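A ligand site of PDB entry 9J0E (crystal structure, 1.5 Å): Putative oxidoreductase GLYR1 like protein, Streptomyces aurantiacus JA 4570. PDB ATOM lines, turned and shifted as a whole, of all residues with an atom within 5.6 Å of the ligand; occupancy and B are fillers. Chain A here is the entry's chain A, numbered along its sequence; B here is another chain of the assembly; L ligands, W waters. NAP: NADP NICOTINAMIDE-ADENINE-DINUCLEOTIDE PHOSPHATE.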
ATOM      1  N   GLY A   9     -11.052   1.511  -2.241  1.00  0.00           N
ATOM      2  CA  GLY A   9     -11.767   2.735  -2.553  1.00  0.00           C
ATOM      3  C   GLY A   9     -11.609   3.117  -4.005  1.00  0.00           C
ATOM      4  O   GLY A   9     -10.504   3.404  -4.472  1.00  0.00           O
ATOM      5  N   LEU A  10     -12.718   3.130  -4.746  1.00  0.00           N
ATOM      6  CA  LEU A  10     -12.714   3.462  -6.164  1.00  0.00           C
ATOM      7  C   LEU A  10     -13.557   4.688  -6.455  1.00  0.00           C
ATOM      8  O   LEU A  10     -14.226   4.780  -7.489  1.00  0.00           O
ATOM      9  CB  LEU A  10     -13.113   2.272  -7.035  1.00  0.00           C
ATOM     10  CG  LEU A  10     -12.113   1.104  -6.993  1.00  0.00           C
ATOM     11  CD1 LEU A  10     -12.622  -0.064  -7.846  1.00  0.00           C
ATOM     12  CD2 LEU A  10     -10.705   1.539  -7.438  1.00  0.00           C
ATOM     13  N   GLY A  11     -13.579   5.639  -5.522  1.00  0.00           N
ATOM     14  CA  GLY A  11     -14.002   6.979  -5.836  1.00  0.00           C
ATOM     15  C   GLY A  11     -13.020   7.613  -6.807  1.00  0.00           C
ATOM     16  O   GLY A  11     -12.097   6.976  -7.329  1.00  0.00           O
ATOM     17  N   ALA A  12     -13.222   8.907  -7.056  1.00  0.00           N
ATOM     18  CA  ALA A  12     -12.351   9.613  -7.995  1.00  0.00           C
ATOM     19  C   ALA A  12     -10.891   9.495  -7.585  1.00  0.00           C
ATOM     20  O   ALA A  12     -10.028   9.212  -8.420  1.00  0.00           O
ATOM     21  CB  ALA A  12     -12.765  11.086  -8.094  1.00  0.00           C
ATOM     22  N   MET A  13     -10.596   9.709  -6.307  1.00  0.00           N
ATOM     23  CA  MET A  13      -9.191   9.701  -5.911  1.00  0.00           C
ATOM     24  C   MET A  13      -8.608   8.288  -5.824  1.00  0.00           C
ATOM     25  O   MET A  13      -7.482   8.055  -6.266  1.00  0.00           O
ATOM     26  CB  MET A  13      -9.005  10.482  -4.611  1.00  0.00           C
ATOM     27  CG  MET A  13      -7.547  10.607  -4.166  1.00  0.00           C
ATOM     28  SD  MET A  13      -6.413  11.247  -5.431  1.00  0.00           S
ATOM     29  CE  MET A  13      -6.733  13.019  -5.348  1.00  0.00           C
ATOM     30  N   GLY A  14      -9.353   7.331  -5.273  1.00  0.00           N
ATOM     31  CA  GLY A  14      -8.867   5.954  -5.292  1.00  0.00           C
ATOM     32  C   GLY A  14      -8.541   5.470  -6.687  1.00  0.00           C
ATOM     33  O   GLY A  14      -7.529   4.783  -6.900  1.00  0.00           O
ATOM     34  N   TRP A  31     -10.479  -2.689  -4.934  1.00  0.00           N
ATOM     35  CA  TRP A  31     -11.726  -3.087  -4.295  1.00  0.00           C
ATOM     36  C   TRP A  31     -12.553  -1.836  -3.982  1.00  0.00           C
ATOM     37  O   TRP A  31     -11.993  -0.782  -3.646  1.00  0.00           O
ATOM     38  CB  TRP A  31     -11.466  -3.854  -2.999  1.00  0.00           C
ATOM     39  CG  TRP A  31     -12.726  -4.283  -2.328  1.00  0.00           C
ATOM     40  CD1 TRP A  31     -13.401  -5.465  -2.511  1.00  0.00           C
ATOM     41  CD2 TRP A  31     -13.476  -3.556  -1.353  1.00  0.00           C
ATOM     42  NE1 TRP A  31     -14.525  -5.502  -1.728  1.00  0.00           N
ATOM     43  CE2 TRP A  31     -14.597  -4.337  -1.004  1.00  0.00           C
ATOM     44  CE3 TRP A  31     -13.321  -2.297  -0.751  1.00  0.00           C
ATOM     45  CZ2 TRP A  31     -15.552  -3.912  -0.073  1.00  0.00           C
ATOM     46  CZ3 TRP A  31     -14.263  -1.883   0.177  1.00  0.00           C
ATOM     47  CH2 TRP A  31     -15.367  -2.684   0.505  1.00  0.00           C
ATOM     48  N   ASN A  32     -13.874  -1.955  -4.094  1.00  0.00           N
ATOM     49  CA  ASN A  32     -14.772  -0.874  -3.709  1.00  0.00           C
ATOM     50  C   ASN A  32     -16.055  -1.482  -3.151  1.00  0.00           C
ATOM     51  O   ASN A  32     -16.459  -2.569  -3.565  1.00  0.00           O
ATOM     52  CB  ASN A  32     -15.096   0.041  -4.903  1.00  0.00           C
ATOM     53  CG  ASN A  32     -15.805   1.331  -4.486  1.00  0.00           C
ATOM     54  OD1 ASN A  32     -15.229   2.155  -3.766  1.00  0.00           O
ATOM     55  ND2 ASN A  32     -17.046   1.505  -4.950  1.00  0.00           N
ATOM     56  N   ARG A  33     -16.662  -0.770  -2.209  1.00  0.00           N
ATOM     57  CA  ARG A  33     -17.938  -1.231  -1.641  1.00  0.00           C
ATOM     58  C   ARG A  33     -18.971  -1.448  -2.736  1.00  0.00           C
ATOM     59  O   ARG A  33     -19.588  -2.521  -2.824  1.00  0.00           O
ATOM     60  CB  ARG A  33     -18.442  -0.217  -0.615  1.00  0.00           C
ATOM     61  CG  ARG A  33     -19.906  -0.441  -0.202  1.00  0.00           C
ATOM     62  CD  ARG A  33     -20.379   0.625   0.788  1.00  0.00           C
ATOM     63  NE  ARG A  33     -20.396   1.965   0.203  1.00  0.00           N
ATOM     64  CZ  ARG A  33     -20.957   3.015   0.778  1.00  0.00           C
ATOM     65  NH1 ARG A  33     -21.549   2.939   1.960  1.00  0.00           N
ATOM     66  NH2 ARG A  33     -20.930   4.188   0.150  1.00  0.00           N
ATOM     67  N   SER A  34     -19.198  -0.431  -3.568  1.00  0.00           N
ATOM     68  CA  SER A  34     -20.241  -0.467  -4.594  1.00  0.00           C
ATOM     69  C   SER A  34     -19.667  -1.017  -5.896  1.00  0.00           C
ATOM     70  O   SER A  34     -18.569  -0.635  -6.292  1.00  0.00           O
ATOM     71  CB  SER A  34     -20.792   0.939  -4.835  1.00  0.00           C
ATOM     72  OG  SER A  34     -21.413   1.430  -3.665  1.00  0.00           O
ATOM     73  N   LYS A  37     -17.369   0.083 -10.664  1.00  0.00           N
ATOM     74  CA  LYS A  37     -16.568   1.280 -10.854  1.00  0.00           C
ATOM     75  C   LYS A  37     -15.171   0.923 -11.374  1.00  0.00           C
ATOM     76  O   LYS A  37     -14.664  -0.176 -11.145  1.00  0.00           O
ATOM     77  CB  LYS A  37     -16.447   2.054  -9.535  1.00  0.00           C
ATOM     78  CG  LYS A  37     -17.796   2.392  -8.884  1.00  0.00           C
ATOM     79  CD  LYS A  37     -17.680   3.592  -7.947  1.00  0.00           C
ATOM     80  CE  LYS A  37     -17.569   4.910  -8.733  1.00  0.00           C
ATOM     81  NZ  LYS A  37     -16.825   5.978  -7.999  1.00  0.00           N
ATOM     82  N   CYS A  65      -8.478   4.913   0.515  1.00  0.00           N
ATOM     83  CA  CYS A  65      -8.878   6.285   0.171  1.00  0.00           C
ATOM     84  C   CYS A  65     -10.404   6.296   0.009  1.00  0.00           C
ATOM     85  O   CYS A  65     -10.931   6.060  -1.078  1.00  0.00           O
ATOM     86  CB  CYS A  65      -8.175   6.751  -1.082  1.00  0.00           C
ATOM     87  SG  CYS A  65      -8.491   8.482  -1.492  1.00  0.00           S
ATOM     88  N   VAL A  66     -11.094   6.581   1.110  1.00  0.00           N
ATOM     89  CA  VAL A  66     -12.558   6.641   1.110  1.00  0.00           C
ATOM     90  C   VAL A  66     -12.986   7.963   1.744  1.00  0.00           C
ATOM     91  O   VAL A  66     -12.151   8.846   1.966  1.00  0.00           O
ATOM     92  CB  VAL A  66     -13.185   5.410   1.792  1.00  0.00           C
ATOM     93  CG1 VAL A  66     -12.904   4.153   0.971  1.00  0.00           C
ATOM     94  CG2 VAL A  66     -12.637   5.243   3.212  1.00  0.00           C
ATOM     95  N   VAL A  67     -14.277   8.133   2.034  1.00  0.00           N
ATOM     96  CA  VAL A  67     -14.743   9.476   2.383  1.00  0.00           C
ATOM     97  C   VAL A  67     -14.395   9.879   3.822  1.00  0.00           C
ATOM     98  O   VAL A  67     -14.206  11.072   4.104  1.00  0.00           O
ATOM     99  CB  VAL A  67     -16.232   9.646   2.078  1.00  0.00           C
ATOM    100  CG1 VAL A  67     -17.082   8.973   3.143  1.00  0.00           C
ATOM    101  CG2 VAL A  67     -16.589  11.131   1.945  1.00  0.00           C
ATOM    102  N   ASP A  68     -14.312   8.937   4.752  1.00  0.00           N
ATOM    103  CA  ASP A  68     -14.040   9.276   6.152  1.00  0.00           C
ATOM    104  C   ASP A  68     -13.570   8.023   6.877  1.00  0.00           C
ATOM    105  O   ASP A  68     -13.531   6.925   6.317  1.00  0.00           O
ATOM    106  CB  ASP A  68     -15.230   9.980   6.821  1.00  0.00           C
ATOM    107  CG  ASP A  68     -16.497   9.129   6.872  1.00  0.00           C
ATOM    108  OD1 ASP A  68     -16.419   7.883   6.836  1.00  0.00           O
ATOM    109  OD2 ASP A  68     -17.592   9.734   6.951  1.00  0.00           O
ATOM    110  N   GLU A  70     -15.021   6.653   9.614  1.00  0.00           N
ATOM    111  CA  GLU A  70     -16.110   5.714   9.869  1.00  0.00           C
ATOM    112  C   GLU A  70     -16.152   4.682   8.751  1.00  0.00           C
ATOM    113  O   GLU A  70     -16.304   3.476   9.005  1.00  0.00           O
ATOM    114  CB  GLU A  70     -17.440   6.451   9.989  1.00  0.00           C
ATOM    115  CG  GLU A  70     -18.558   5.643  10.693  1.00  0.00           C
ATOM    116  CD  GLU A  70     -19.174   4.527   9.824  1.00  0.00           C
ATOM    117  OE1 GLU A  70     -19.298   4.700   8.591  1.00  0.00           O
ATOM    118  OE2 GLU A  70     -19.540   3.476  10.403  1.00  0.00           O
ATOM    119  N   ALA A  71     -15.995   5.137   7.502  1.00  0.00           N
ATOM    120  CA  ALA A  71     -15.977   4.220   6.365  1.00  0.00           C
ATOM    121  C   ALA A  71     -14.715   3.347   6.371  1.00  0.00           C
ATOM    122  O   ALA A  71     -14.816   2.115   6.293  1.00  0.00           O
ATOM    123  CB  ALA A  71     -16.113   5.000   5.053  1.00  0.00           C
ATOM    124  N   SER A  74     -14.738   0.729   9.130  1.00  0.00           N
ATOM    125  CA  SER A  74     -15.761  -0.298   8.927  1.00  0.00           C
ATOM    126  C   SER A  74     -15.278  -1.363   7.939  1.00  0.00           C
ATOM    127  O   SER A  74     -15.702  -2.525   8.026  1.00  0.00           O
ATOM    128  CB  SER A  74     -17.080   0.336   8.459  1.00  0.00           C
ATOM    129  OG  SER A  74     -17.033   0.717   7.099  1.00  0.00           O
ATOM    130  N   ILE A  75     -14.419  -0.986   6.995  1.00  0.00           N
ATOM    131  CA  ILE A  75     -13.819  -1.935   6.058  1.00  0.00           C
ATOM    132  C   ILE A  75     -12.697  -2.704   6.727  1.00  0.00           C
ATOM    133  O   ILE A  75     -12.571  -3.924   6.539  1.00  0.00           O
ATOM    134  CB  ILE A  75     -13.302  -1.195   4.812  1.00  0.00           C
ATOM    135  CG1 ILE A  75     -14.405  -0.446   4.066  1.00  0.00           C
ATOM    136  CG2 ILE A  75     -12.576  -2.166   3.883  1.00  0.00           C
ATOM    137  CD1 ILE A  75     -13.839   0.645   3.136  1.00  0.00           C
ATOM    138  N   VAL A  91      -4.941   7.279   3.296  1.00  0.00           N
ATOM    139  CA  VAL A  91      -4.820   8.668   2.861  1.00  0.00           C
ATOM    140  C   VAL A  91      -6.174   9.370   2.822  1.00  0.00           C
ATOM    141  O   VAL A  91      -6.296  10.453   2.235  1.00  0.00           O
ATOM    142  CB  VAL A  91      -4.049   8.831   1.547  1.00  0.00           C
ATOM    143  CG1 VAL A  91      -2.582   8.390   1.700  1.00  0.00           C
ATOM    144  CG2 VAL A  91      -4.724   8.081   0.394  1.00  0.00           C
ATOM    145  N   THR A  92      -7.209   8.773   3.420  1.00  0.00           N
ATOM    146  CA  THR A  92      -8.490   9.451   3.599  1.00  0.00           C
ATOM    147  C   THR A  92      -8.300  10.719   4.428  1.00  0.00           C
ATOM    148  O   THR A  92      -7.621  10.701   5.456  1.00  0.00           O
ATOM    149  CB  THR A  92      -9.424   8.496   4.366  1.00  0.00           C
ATOM    150  OG1 THR A  92      -9.635   7.303   3.590  1.00  0.00           O
ATOM    151  CG2 THR A  92     -10.770   9.141   4.684  1.00  0.00           C
ATOM    152  N   SER A  93      -8.899  11.830   3.981  1.00  0.00           N
ATOM    153  CA  SER A  93      -8.794  13.090   4.725  1.00  0.00           C
ATOM    154  C   SER A  93      -9.776  13.093   5.895  1.00  0.00           C
ATOM    155  O   SER A  93     -10.985  12.966   5.693  1.00  0.00           O
ATOM    156  CB  SER A  93      -9.045  14.294   3.822  1.00  0.00           C
ATOM    157  OG  SER A  93      -8.954  15.492   4.576  1.00  0.00           O
ATOM    158  N   VAL A 118      -3.764  13.222   0.610  1.00  0.00           N
ATOM    159  CA  VAL A 118      -3.549  13.672  -0.766  1.00  0.00           C
ATOM    160  C   VAL A 118      -3.928  15.149  -0.836  1.00  0.00           C
ATOM    161  O   VAL A 118      -5.071  15.511  -0.550  1.00  0.00           O
ATOM    162  CB  VAL A 118      -4.403  12.869  -1.757  1.00  0.00           C
ATOM    163  CG1 VAL A 118      -4.091  13.302  -3.190  1.00  0.00           C
ATOM    164  CG2 VAL A 118      -4.189  11.367  -1.566  1.00  0.00           C
ATOM    165  N   MET A 119      -2.976  16.005  -1.216  1.00  0.00           N
ATOM    166  CA  MET A 119      -3.185  17.446  -1.137  1.00  0.00           C
ATOM    167  C   MET A 119      -3.511  18.093  -2.480  1.00  0.00           C
ATOM    168  O   MET A 119      -3.670  19.318  -2.535  1.00  0.00           O
ATOM    169  CB  MET A 119      -1.971  18.123  -0.500  1.00  0.00           C
ATOM    170  CG  MET A 119      -1.615  17.570   0.879  1.00  0.00           C
ATOM    171  SD  MET A 119      -3.037  17.405   2.001  1.00  0.00           S
ATOM    172  CE  MET A 119      -3.638  19.087   2.012  1.00  0.00           C
ATOM    173  N   ILE A 120      -3.631  17.323  -3.556  1.00  0.00           N
ATOM    174  CA  ILE A 120      -3.818  17.860  -4.895  1.00  0.00           C
ATOM    175  C   ILE A 120      -4.958  17.135  -5.605  1.00  0.00           C
ATOM    176  O   ILE A 120      -5.399  16.070  -5.151  1.00  0.00           O
ATOM    177  CB  ILE A 120      -2.504  17.834  -5.703  1.00  0.00           C
ATOM    178  CG1 ILE A 120      -1.734  16.525  -5.497  1.00  0.00           C
ATOM    179  CG2 ILE A 120      -1.627  18.997  -5.282  1.00  0.00           C
ATOM    180  CD1 ILE A 120      -2.387  15.281  -6.093  1.00  0.00           C
ATOM    181  N   PRO A 121      -5.462  17.675  -6.708  1.00  0.00           N
ATOM    182  CA  PRO A 121      -6.554  17.010  -7.439  1.00  0.00           C
ATOM    183  C   PRO A 121      -6.073  15.771  -8.192  1.00  0.00           C
ATOM    184  O   PRO A 121      -4.882  15.525  -8.390  1.00  0.00           O
ATOM    185  CB  PRO A 121      -7.063  18.085  -8.402  1.00  0.00           C
ATOM    186  CG  PRO A 121      -5.973  19.112  -8.470  1.00  0.00           C
ATOM    187  CD  PRO A 121      -5.178  19.026  -7.206  1.00  0.00           C
ATOM    188  N   THR A 122      -7.072  14.981  -8.638  1.00  0.00           N
ATOM    189  CA  THR A 122      -6.771  13.666  -9.209  1.00  0.00           C
ATOM    190  C   THR A 122      -5.827  13.731 -10.394  1.00  0.00           C
ATOM    191  O   THR A 122      -4.986  12.838 -10.580  1.00  0.00           O
ATOM    192  CB  THR A 122      -8.050  12.931  -9.585  1.00  0.00           C
ATOM    193  OG1 THR A 122      -8.766  13.693 -10.566  1.00  0.00           O
ATOM    194  CG2 THR A 122      -8.935  12.682  -8.355  1.00  0.00           C
ATOM    195  N   LEU A 173      -6.259  22.460   4.020  1.00  0.00           N
ATOM    196  CA  LEU A 173      -7.607  22.470   3.439  1.00  0.00           C
ATOM    197  C   LEU A 173      -8.458  23.591   4.019  1.00  0.00           C
ATOM    198  O   LEU A 173      -9.323  24.126   3.322  1.00  0.00           O
ATOM    199  CB  LEU A 173      -8.299  21.130   3.659  1.00  0.00           C
ATOM    200  CG  LEU A 173      -7.708  19.910   2.961  1.00  0.00           C
ATOM    201  CD1 LEU A 173      -8.560  18.700   3.309  1.00  0.00           C
ATOM    202  CD2 LEU A 173      -7.635  20.086   1.468  1.00  0.00           C
ATOM    203  N   GLU B 231     -14.342  14.493 -11.114  1.00  0.00           N
ATOM    204  CA  GLU B 231     -13.065  14.236 -10.464  1.00  0.00           C
ATOM    205  C   GLU B 231     -12.993  14.787  -9.047  1.00  0.00           C
ATOM    206  O   GLU B 231     -11.996  14.551  -8.357  1.00  0.00           O
ATOM    207  CB  GLU B 231     -11.914  14.803 -11.308  1.00  0.00           C
ATOM    208  CG  GLU B 231     -11.744  14.114 -12.650  1.00  0.00           C
ATOM    209  CD  GLU B 231     -11.479  12.624 -12.517  1.00  0.00           C
ATOM    210  OE1 GLU B 231     -10.814  12.207 -11.532  1.00  0.00           O
ATOM    211  OE2 GLU B 231     -11.928  11.852 -13.391  1.00  0.00           O
ATOM    212  N   ALA B 232     -13.997  15.535  -8.612  1.00  0.00           N
ATOM    213  CA  ALA B 232     -14.024  16.083  -7.264  1.00  0.00           C
ATOM    214  C   ALA B 232     -15.428  16.603  -6.977  1.00  0.00           C
ATOM    215  O   ALA B 232     -15.746  17.732  -7.346  1.00  0.00           O
ATOM    216  CB  ALA B 232     -13.004  17.218  -7.116  1.00  0.00           C
ATOM    217  N   ASN B 233     -16.268  15.777  -6.359  1.00  0.00           N
ATOM    218  CA  ASN B 233     -17.667  16.135  -6.228  1.00  0.00           C
ATOM    219  C   ASN B 233     -17.941  16.911  -4.947  1.00  0.00           C
ATOM    220  O   ASN B 233     -17.221  16.788  -3.943  1.00  0.00           O
ATOM    221  CB  ASN B 233     -18.591  14.926  -6.387  1.00  0.00           C
ATOM    222  CG  ASN B 233     -18.467  13.910  -5.250  1.00  0.00           C
ATOM    223  OD1 ASN B 233     -18.918  14.169  -4.142  1.00  0.00           O
ATOM    224  ND2 ASN B 233     -17.895  12.749  -5.544  1.00  0.00           N
ATOM    225  N   MET B 236     -18.413  15.126  -1.553  1.00  0.00           N
ATOM    226  CA  MET B 236     -17.142  14.788  -0.916  1.00  0.00           C
ATOM    227  C   MET B 236     -16.520  16.013  -0.255  1.00  0.00           C
ATOM    228  O   MET B 236     -15.983  15.926   0.864  1.00  0.00           O
ATOM    229  CB  MET B 236     -16.198  14.172  -1.962  1.00  0.00           C
ATOM    230  CG  MET B 236     -14.748  13.914  -1.499  1.00  0.00           C
ATOM    231  SD  MET B 236     -13.739  15.422  -1.625  1.00  0.00           S
ATOM    232  CE  MET B 236     -13.704  15.669  -3.433  1.00  0.00           C
ATOM    233  N   GLY B 240     -15.336  16.832   3.699  1.00  0.00           N
ATOM    234  CA  GLY B 240     -14.003  17.320   4.044  1.00  0.00           C
ATOM    235  C   GLY B 240     -14.067  18.568   4.914  1.00  0.00           C
ATOM    236  O   GLY B 240     -13.328  18.689   5.903  1.00  0.00           O
HETATM  237  PA  NAP L   1     -15.644  10.005  -3.976  1.00  0.00           P
HETATM  238  O1A NAP L   1     -15.351   9.969  -5.436  1.00  0.00           O
HETATM  239  O2A NAP L   1     -16.927  10.590  -3.472  1.00  0.00           O
HETATM  240  O5B NAP L   1     -15.457   8.483  -3.439  1.00  0.00           O
HETATM  241  C5B NAP L   1     -15.879   8.190  -2.125  1.00  0.00           C
HETATM  242  C4B NAP L   1     -15.301   6.824  -1.793  1.00  0.00           C
HETATM  243  O4B NAP L   1     -15.564   6.449  -0.437  1.00  0.00           O
HETATM  244  C3B NAP L   1     -15.883   5.652  -2.642  1.00  0.00           C
HETATM  245  O3B NAP L   1     -14.954   4.631  -2.865  1.00  0.00           O
HETATM  246  C2B NAP L   1     -17.054   5.215  -1.745  1.00  0.00           C
HETATM  247  O2B NAP L   1     -17.427   3.904  -1.996  1.00  0.00           O
HETATM  248  C1B NAP L   1     -16.362   5.274  -0.377  1.00  0.00           C
HETATM  249  N9A NAP L   1     -17.233   5.227   0.787  1.00  0.00           N
HETATM  250  C8A NAP L   1     -18.045   6.188   1.341  1.00  0.00           C
HETATM  251  N7A NAP L   1     -18.693   5.770   2.391  1.00  0.00           N
HETATM  252  C5A NAP L   1     -18.311   4.462   2.527  1.00  0.00           C
HETATM  253  C6A NAP L   1     -18.655   3.465   3.467  1.00  0.00           C
HETATM  254  N6A NAP L   1     -19.503   3.699   4.469  1.00  0.00           N
HETATM  255  N1A NAP L   1     -18.089   2.261   3.332  1.00  0.00           N
HETATM  256  C2A NAP L   1     -17.232   2.038   2.328  1.00  0.00           C
HETATM  257  N3A NAP L   1     -16.830   2.903   1.400  1.00  0.00           N
HETATM  258  C4A NAP L   1     -17.407   4.100   1.546  1.00  0.00           C
HETATM  259  O3  NAP L   1     -14.497  10.792  -3.145  1.00  0.00           O
HETATM  260  PN  NAP L   1     -12.932  10.959  -3.553  1.00  0.00           P
HETATM  261  O1N NAP L   1     -12.792  12.213  -4.339  1.00  0.00           O
HETATM  262  O2N NAP L   1     -12.395   9.681  -4.098  1.00  0.00           O
HETATM  263  O5D NAP L   1     -12.334  11.244  -2.046  1.00  0.00           O
HETATM  264  C5D NAP L   1     -11.661  10.262  -1.299  1.00  0.00           C
HETATM  265  C4D NAP L   1     -10.775  10.974  -0.296  1.00  0.00           C
HETATM  266  O4D NAP L   1      -9.755  11.620  -1.061  1.00  0.00           O
HETATM  267  C3D NAP L   1     -11.469  12.062   0.494  1.00  0.00           C
HETATM  268  O3D NAP L   1     -10.944  11.926   1.807  1.00  0.00           O
HETATM  269  C2D NAP L   1     -10.982  13.364  -0.153  1.00  0.00           C
HETATM  270  O2D NAP L   1     -10.949  14.446   0.720  1.00  0.00           O
HETATM  271  C1D NAP L   1      -9.601  12.916  -0.630  1.00  0.00           C
HETATM  272  N1N NAP L   1      -9.144  13.796  -1.737  1.00  0.00           N
HETATM  273  C2N NAP L   1      -9.842  13.886  -2.877  1.00  0.00           C
HETATM  274  C3N NAP L   1      -9.409  14.720  -3.884  1.00  0.00           C
HETATM  275  C7N NAP L   1     -10.128  14.853  -5.202  1.00  0.00           C
HETATM  276  O7N NAP L   1     -11.040  14.083  -5.534  1.00  0.00           O
HETATM  277  N7N NAP L   1      -9.713  15.838  -5.974  1.00  0.00           N
HETATM  278  C4N NAP L   1      -8.249  15.461  -3.685  1.00  0.00           C
HETATM  279  C5N NAP L   1      -7.559  15.358  -2.498  1.00  0.00           C
HETATM  280  C6N NAP L   1      -8.033  14.506  -1.528  1.00  0.00           C
HETATM  281  P2B NAP L   1     -18.893   3.746  -2.884  1.00  0.00           P
HETATM  282  O1X NAP L   1     -18.468   3.853  -4.334  1.00  0.00           O
HETATM  283  O2X NAP L   1     -19.343   2.349  -2.500  1.00  0.00           O
HETATM  284  O3X NAP L   1     -19.796   4.848  -2.343  1.00  0.00           O
HETATM  285  O   HOH W   1      -9.727  16.211  -8.699  1.00  0.00           O
HETATM  286  O   HOH W   2     -20.004   7.415  -2.271  1.00  0.00           O
HETATM  287  O   HOH W   3     -20.662   4.574  -6.077  1.00  0.00           O
HETATM  288  O   HOH W   4     -11.716   6.971  -3.645  1.00  0.00           O
HETATM  289  O   HOH W   5     -18.830   8.679  -4.285  1.00  0.00           O
HETATM  290  O   HOH W   6     -22.464   4.741  -3.137  1.00  0.00           O
HETATM  291  O   HOH W   7     -20.326   6.935   4.288  1.00  0.00           O
HETATM  292  O   HOH W   8     -12.637  13.170   3.591  1.00  0.00           O
HETATM  293  O   HOH W   9     -18.584  -0.070   4.765  1.00  0.00           O
HETATM  294  O   HOH W  10     -17.797   6.339  -5.528  1.00  0.00           O
HETATM  295  O   HOH W  11     -13.388  15.080   1.698  1.00  0.00           O
HETATM  296  O   HOH W  12      -9.191  16.525   0.708  1.00  0.00           O
HETATM  297  O   HOH W  13     -14.865  13.216  -5.919  1.00  0.00           O
HETATM  298  O   HOH W  14     -15.471   1.525  -0.917  1.00  0.00           O
HETATM  299  O   HOH W  15     -16.890   9.500  -7.506  1.00  0.00           O
HETATM  300  O   HOH W  16     -19.631   2.264   7.037  1.00  0.00           O
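OD1 of Asn 32 is in hydrogen-bond range of N of Leu 10. OE1 of Glu 231 of chain B sits at hydrogen-bond distance from OG1 of Thr 122 (2.7 Å). The backbone NH (N) of Met 236 of chain B is in hydrogen-bond range of the side-chain amide oxygen (OD1) of Asn 233 of chain B (2.8 Å). NZ of Lys 37 lies within hydrogen-bond range of O of Leu 10 (2.9 Å). The backbone NH (N) of Val 66 is in hydrogen-bond range of the side-chain hydroxyl (OG1) of Thr 92 (3.0 Å). The side-chain hydroxyl of Ser 74 is in hydrogen-bond range of the backbone carbonyl oxygen of Ala 71, 2.7 Å away. N of Ala 71 sits at hydrogen-bond distance from OD1 of Asp 68 (2.9 Å). O of Trp 31 lies within hydrogen-bond range of N of Gly 9 (2.8 Å).
Water W11 lies within hydrogen-bond range of an oxygen (O2D) of the ligand (2.7 Å), the backbone carbonyl oxygen (O) of Met 236 of chain B (2.9 Å) and the backbone NH (N) of Gly 240 of chain B (3.3 Å). Water W1 lies within hydrogen-bond range of a nitrogen (N7N) of the ligand (2.8 Å), the backbone carbonyl oxygen (O) of Glu 231 of chain B (2.8 Å) and the backbone NH (N) of Thr 122 (2.9 Å). Water W8 lies within hydrogen-bond range of O of Val 67 (2.7 Å), O of Ser 93 (2.7 Å) and O3D of the ligand (2.8 Å). Water W9 bridges N1A of the ligand (2.8 Å) and OG of Ser 74 (2.9 Å). Water W4 lies within hydrogen-bond range of O2N of the ligand (2.8 Å), O of Cys 65 (2.8 Å), N of Gly 14 (2.9 Å) and N of Gly 11 (3.0 Å). Water W16 lies within hydrogen-bond range of the side-chain carboxylate (OE1) of Glu 70 (2.9 Å), a nitrogen (N6A) of the ligand (2.9 Å) and the side-chain hydroxyl (OG) of Ser 74 (3.0 Å).
An oxygen (O2X) of the ligand sits at hydrogen-bond distance from the backbone NH of Ser 34, at 3.0 Å. An oxygen (O2X) of the ligand lies within hydrogen-bond range of the side-chain hydroxyl of Ser 34, 2.5 Å away. OD1 of Asn 32 sits at hydrogen-bond distance from O3B of the ligand (2.6 Å). NH2 of Arg 33 is in salt-bridge range of O3X of the ligand, at 2.8 Å. N of Met 13 lies within hydrogen-bond range of O2N of the ligand (2.8 Å). N of Ala 12 lies within hydrogen-bond range of O1A of the ligand. N of Ser 93 is in hydrogen-bond range of O3D of the ligand (3.0 Å). O2A of the ligand is in hydrogen-bond range of ND2 of Asn 233 of chain B, 3.1 Å away. O3B of the ligand lies within hydrogen-bond range of N of Gly 11 (3.2 Å). The backbone NH (N) of Val 67 lies within hydrogen-bond range of an oxygen (O4B) of the ligand (3.3 Å). O3B of the ligand is in hydrogen-bond range of N of Leu 10, 3.3 Å away. An oxygen (O3D) of the ligand is in hydrogen-bond range of the backbone carbonyl oxygen (O) of Val 66 (3.3 Å). The side-chain sulfur (SG) of Cys 65 sits at hydrogen-bond distance from an oxygen (O4D) of the ligand (3.4 Å). An oxygen (O2D) of the ligand lies close to the side-chain sulfur (SD) of Met 236 of chain B (3.8 Å).
The backbone carbonyl oxygen (O) of Glu 231 of chain B sits close to an oxygen (O7N) of the ligand (3.0 Å). Residues that only touch the ligand: Gly 9 (3.7 Å), Lys 37 (3.7 Å), Ala 71 (3.4 Å), Ile 75 (3.8 Å), Thr 92 (3.9 Å), Val 118 (3.2 Å), Ile 120 (3.3 Å), Pro 121 (3.7 Å), Thr 122 (3.8 Å) and Ala 232 of chain B (3.7 Å). Hydrophobic or aromatic side chains that line the ligand: Ala 12, Met 13, Val 66, Val 67, Ala 71, Ile 75, Val 118, Ala 232 of chain B and Met 236 of chain B. 24 residues have an atom within 4 Å of the ligand: Gly 9, Leu 10, Gly 11, Ala 12, Met 13, Asn 32, Arg 33, Ser 34, Lys 37, Cys 65, Val 66, Val 67, Ala 71, Ile 75, Thr 92, Ser 93, Val 118, Ile 120, Pro 121, Thr 122, Glu 231 of chain B, Ala 232 of chain B, Asn 233 of chain B and Met 236 of chain B. The nearest printed residue that does not touch the ligand is Gly 14 (4.02 Å).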
